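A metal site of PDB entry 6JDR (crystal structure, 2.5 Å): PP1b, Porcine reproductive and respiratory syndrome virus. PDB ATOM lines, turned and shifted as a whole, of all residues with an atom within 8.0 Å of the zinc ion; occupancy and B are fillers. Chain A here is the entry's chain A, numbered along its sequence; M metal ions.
OG1 of Thr 61 sits at hydrogen-bond distance from NE2 of His 28, at 3.3 Å.
N of Ala 12 lies close to SG of Cys 10, at 3.6 Å.
SG of Cys 7 sits close to N of Tyr 9 (3.4 Å).
N of Cys 7 is in hydrogen-bond range of O of Ala 12.
N of Tyr 27 lies close to SG of Cys 25, at 3.8 Å.
Four residues have an atom within 4 Å of the zinc ion: Cys 7, Cys 10, Cys 25 and His 28.
The nearest printed residue that does not touch the zinc ion is Tyr 9 (4.2 Å).
A ring nitrogen (ND1) of His 28 binds the zinc ion, at 2.1 Å.
SG of Cys 10 binds the zinc ion.
The zinc ion is bound by SG of Cys 7, 2.3 Å away.
SG of Cys 25 is bound to the zinc ion (2.3 Å).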
ATOM      1  N   MET A   6      30.253  15.327 -28.009  1.00  0.00           N
ATOM      2  CA  MET A   6      30.302  16.674 -28.590  1.00  0.00           C
ATOM      3  C   MET A   6      29.067  16.921 -29.455  1.00  0.00           C
ATOM      4  O   MET A   6      28.504  15.996 -30.033  1.00  0.00           O
ATOM      5  CB  MET A   6      31.582  16.842 -29.409  1.00  0.00           C
ATOM      6  CG  MET A   6      32.856  16.423 -28.686  1.00  0.00           C
ATOM      7  SD  MET A   6      33.113  17.225 -27.081  1.00  0.00           S
ATOM      8  CE  MET A   6      34.226  18.553 -27.518  1.00  0.00           C
ATOM      9  N   CYS A   7      28.673  18.198 -29.553  1.00  0.00           N
ATOM     10  CA  CYS A   7      27.493  18.605 -30.303  1.00  0.00           C
ATOM     11  C   CYS A   7      27.644  18.321 -31.801  1.00  0.00           C
ATOM     12  O   CYS A   7      28.684  18.601 -32.379  1.00  0.00           O
ATOM     13  CB  CYS A   7      27.218  20.095 -30.083  1.00  0.00           C
ATOM     14  SG  CYS A   7      25.749  20.739 -30.918  1.00  0.00           S
ATOM     15  N   GLY A   8      26.595  17.776 -32.406  1.00  0.00           N
ATOM     16  CA  GLY A   8      26.577  17.476 -33.831  1.00  0.00           C
ATOM     17  C   GLY A   8      26.556  18.708 -34.717  1.00  0.00           C
ATOM     18  O   GLY A   8      26.945  18.634 -35.880  1.00  0.00           O
ATOM     19  N   TYR A   9      26.074  19.833 -34.181  1.00  0.00           N
ATOM     20  CA  TYR A   9      26.064  21.104 -34.908  1.00  0.00           C
ATOM     21  C   TYR A   9      27.405  21.818 -34.784  1.00  0.00           C
ATOM     22  O   TYR A   9      28.081  22.082 -35.796  1.00  0.00           O
ATOM     23  CB  TYR A   9      24.978  22.032 -34.382  1.00  0.00           C
ATOM     24  CG  TYR A   9      23.551  21.602 -34.649  1.00  0.00           C
ATOM     25  CD1 TYR A   9      23.044  21.579 -35.950  1.00  0.00           C
ATOM     26  CD2 TYR A   9      22.699  21.237 -33.618  1.00  0.00           C
ATOM     27  CE1 TYR A   9      21.742  21.199 -36.205  1.00  0.00           C
ATOM     28  CE2 TYR A   9      21.393  20.866 -33.858  1.00  0.00           C
ATOM     29  CZ  TYR A   9      20.916  20.842 -35.159  1.00  0.00           C
ATOM     30  OH  TYR A   9      19.614  20.462 -35.413  1.00  0.00           O
ATOM     31  N   CYS A  10      27.797  22.111 -33.541  1.00  0.00           N
ATOM     32  CA  CYS A  10      28.897  23.045 -33.256  1.00  0.00           C
ATOM     33  C   CYS A  10      30.130  22.436 -32.572  1.00  0.00           C
ATOM     34  O   CYS A  10      31.132  23.132 -32.386  1.00  0.00           O
ATOM     35  CB  CYS A  10      28.382  24.185 -32.379  1.00  0.00           C
ATOM     36  SG  CYS A  10      27.919  23.645 -30.711  1.00  0.00           S
ATOM     37  N   GLY A  11      30.061  21.175 -32.172  1.00  0.00           N
ATOM     38  CA  GLY A  11      31.196  20.505 -31.536  1.00  0.00           C
ATOM     39  C   GLY A  11      31.409  20.792 -30.051  1.00  0.00           C
ATOM     40  O   GLY A  11      32.322  20.241 -29.449  1.00  0.00           O
ATOM     41  N   ALA A  12      30.569  21.640 -29.452  1.00  0.00           N
ATOM     42  CA  ALA A  12      30.653  21.918 -28.012  1.00  0.00           C
ATOM     43  C   ALA A  12      30.222  20.691 -27.214  1.00  0.00           C
ATOM     44  O   ALA A  12      29.609  19.780 -27.778  1.00  0.00           O
ATOM     45  CB  ALA A  12      29.770  23.111 -27.666  1.00  0.00           C
ATOM     46  N   PRO A  13      30.536  20.639 -25.900  1.00  0.00           N
ATOM     47  CA  PRO A  13      30.094  19.512 -25.076  1.00  0.00           C
ATOM     48  C   PRO A  13      28.582  19.296 -25.114  1.00  0.00           C
ATOM     49  O   PRO A  13      27.822  20.256 -25.039  1.00  0.00           O
ATOM     50  CB  PRO A  13      30.556  19.915 -23.663  1.00  0.00           C
ATOM     51  CG  PRO A  13      31.742  20.784 -23.903  1.00  0.00           C
ATOM     52  CD  PRO A  13      31.416  21.555 -25.152  1.00  0.00           C
ATOM     53  N   ALA A  14      28.163  18.028 -25.218  1.00  0.00           N
ATOM     54  CA  ALA A  14      26.765  17.692 -25.494  1.00  0.00           C
ATOM     55  C   ALA A  14      26.184  16.741 -24.452  1.00  0.00           C
ATOM     56  O   ALA A  14      26.323  15.519 -24.590  1.00  0.00           O
ATOM     57  CB  ALA A  14      26.648  17.074 -26.888  1.00  0.00           C
ATOM     58  N   ASP A  23      23.602  14.281 -31.047  1.00  0.00           N
ATOM     59  CA  ASP A  23      24.106  14.894 -29.807  1.00  0.00           C
ATOM     60  C   ASP A  23      24.060  16.410 -29.921  1.00  0.00           C
ATOM     61  O   ASP A  23      24.493  16.964 -30.923  1.00  0.00           O
ATOM     62  CB  ASP A  23      25.554  14.479 -29.541  1.00  0.00           C
ATOM     63  CG  ASP A  23      25.689  13.023 -29.167  1.00  0.00           C
ATOM     64  OD1 ASP A  23      24.839  12.523 -28.391  1.00  0.00           O
ATOM     65  OD2 ASP A  23      26.652  12.377 -29.625  1.00  0.00           O
ATOM     66  N   VAL A  24      23.539  17.069 -28.893  1.00  0.00           N
ATOM     67  CA  VAL A  24      23.418  18.524 -28.898  1.00  0.00           C
ATOM     68  C   VAL A  24      23.861  19.156 -27.580  1.00  0.00           C
ATOM     69  O   VAL A  24      23.702  18.573 -26.502  1.00  0.00           O
ATOM     70  CB  VAL A  24      21.977  18.975 -29.219  1.00  0.00           C
ATOM     71  CG1 VAL A  24      21.651  18.714 -30.692  1.00  0.00           C
ATOM     72  CG2 VAL A  24      20.959  18.310 -28.320  1.00  0.00           C
ATOM     73  N   CYS A  25      24.410  20.350 -27.697  1.00  0.00           N
ATOM     74  CA  CYS A  25      24.787  21.158 -26.541  1.00  0.00           C
ATOM     75  C   CYS A  25      23.562  21.895 -26.035  1.00  0.00           C
ATOM     76  O   CYS A  25      22.501  21.874 -26.677  1.00  0.00           O
ATOM     77  CB  CYS A  25      25.870  22.159 -26.939  1.00  0.00           C
ATOM     78  SG  CYS A  25      25.329  23.384 -28.149  1.00  0.00           S
ATOM     79  N   VAL A  26      23.710  22.566 -24.899  1.00  0.00           N
ATOM     80  CA  VAL A  26      22.620  23.256 -24.230  1.00  0.00           C
ATOM     81  C   VAL A  26      21.940  24.255 -25.163  1.00  0.00           C
ATOM     82  O   VAL A  26      20.713  24.353 -25.207  1.00  0.00           O
ATOM     83  CB  VAL A  26      23.126  23.973 -22.948  1.00  0.00           C
ATOM     84  CG1 VAL A  26      22.076  24.922 -22.378  1.00  0.00           C
ATOM     85  CG2 VAL A  26      23.536  22.944 -21.902  1.00  0.00           C
ATOM     86  N   TYR A  27      22.740  25.002 -25.928  1.00  0.00           N
ATOM     87  CA  TYR A  27      22.210  25.997 -26.859  1.00  0.00           C
ATOM     88  C   TYR A  27      21.318  25.344 -27.918  1.00  0.00           C
ATOM     89  O   TYR A  27      20.197  25.779 -28.141  1.00  0.00           O
ATOM     90  CB  TYR A  27      23.356  26.767 -27.515  1.00  0.00           C
ATOM     91  CG  TYR A  27      22.895  27.808 -28.505  1.00  0.00           C
ATOM     92  CD1 TYR A  27      22.270  28.975 -28.070  1.00  0.00           C
ATOM     93  CD2 TYR A  27      23.073  27.632 -29.877  1.00  0.00           C
ATOM     94  CE1 TYR A  27      21.832  29.936 -28.979  1.00  0.00           C
ATOM     95  CE2 TYR A  27      22.641  28.574 -30.787  1.00  0.00           C
ATOM     96  CZ  TYR A  27      22.032  29.735 -30.337  1.00  0.00           C
ATOM     97  OH  TYR A  27      21.607  30.679 -31.240  1.00  0.00           O
ATOM     98  N   HIS A  28      21.819  24.282 -28.543  1.00  0.00           N
ATOM     99  CA  HIS A  28      21.125  23.644 -29.661  1.00  0.00           C
ATOM    100  C   HIS A  28      19.949  22.750 -29.274  1.00  0.00           C
ATOM    101  O   HIS A  28      19.273  22.212 -30.160  1.00  0.00           O
ATOM    102  CB  HIS A  28      22.107  22.875 -30.529  1.00  0.00           C
ATOM    103  CG  HIS A  28      22.946  23.744 -31.400  1.00  0.00           C
ATOM    104  ND1 HIS A  28      24.278  23.987 -31.151  1.00  0.00           N
ATOM    105  CD2 HIS A  28      22.629  24.449 -32.518  1.00  0.00           C
ATOM    106  CE1 HIS A  28      24.751  24.803 -32.090  1.00  0.00           C
ATOM    107  NE2 HIS A  28      23.776  25.092 -32.926  1.00  0.00           N
ATOM    108  N   THR A  29      19.690  22.587 -27.978  1.00  0.00           N
ATOM    109  CA  THR A  29      18.481  21.901 -27.531  1.00  0.00           C
ATOM    110  C   THR A  29      17.196  22.598 -27.999  1.00  0.00           C
ATOM    111  O   THR A  29      16.136  21.992 -28.019  1.00  0.00           O
ATOM    112  CB  THR A  29      18.418  21.770 -25.996  1.00  0.00           C
ATOM    113  OG1 THR A  29      18.650  23.049 -25.386  1.00  0.00           O
ATOM    114  CG2 THR A  29      19.444  20.785 -25.471  1.00  0.00           C
ATOM    115  N   THR A  61      19.733  26.351 -37.272  1.00  0.00           N
ATOM    116  CA  THR A  61      20.987  27.111 -37.395  1.00  0.00           C
ATOM    117  C   THR A  61      21.945  26.478 -38.398  1.00  0.00           C
ATOM    118  O   THR A  61      23.045  27.014 -38.629  1.00  0.00           O
ATOM    119  CB  THR A  61      21.720  27.163 -36.045  1.00  0.00           C
ATOM    120  OG1 THR A  61      22.062  25.844 -35.617  1.00  0.00           O
ATOM    121  CG2 THR A  61      20.842  27.820 -34.996  1.00  0.00           C
HETATM  122 ZN    ZN M   1      25.917  22.936 -30.340  1.00  0.00          ZN
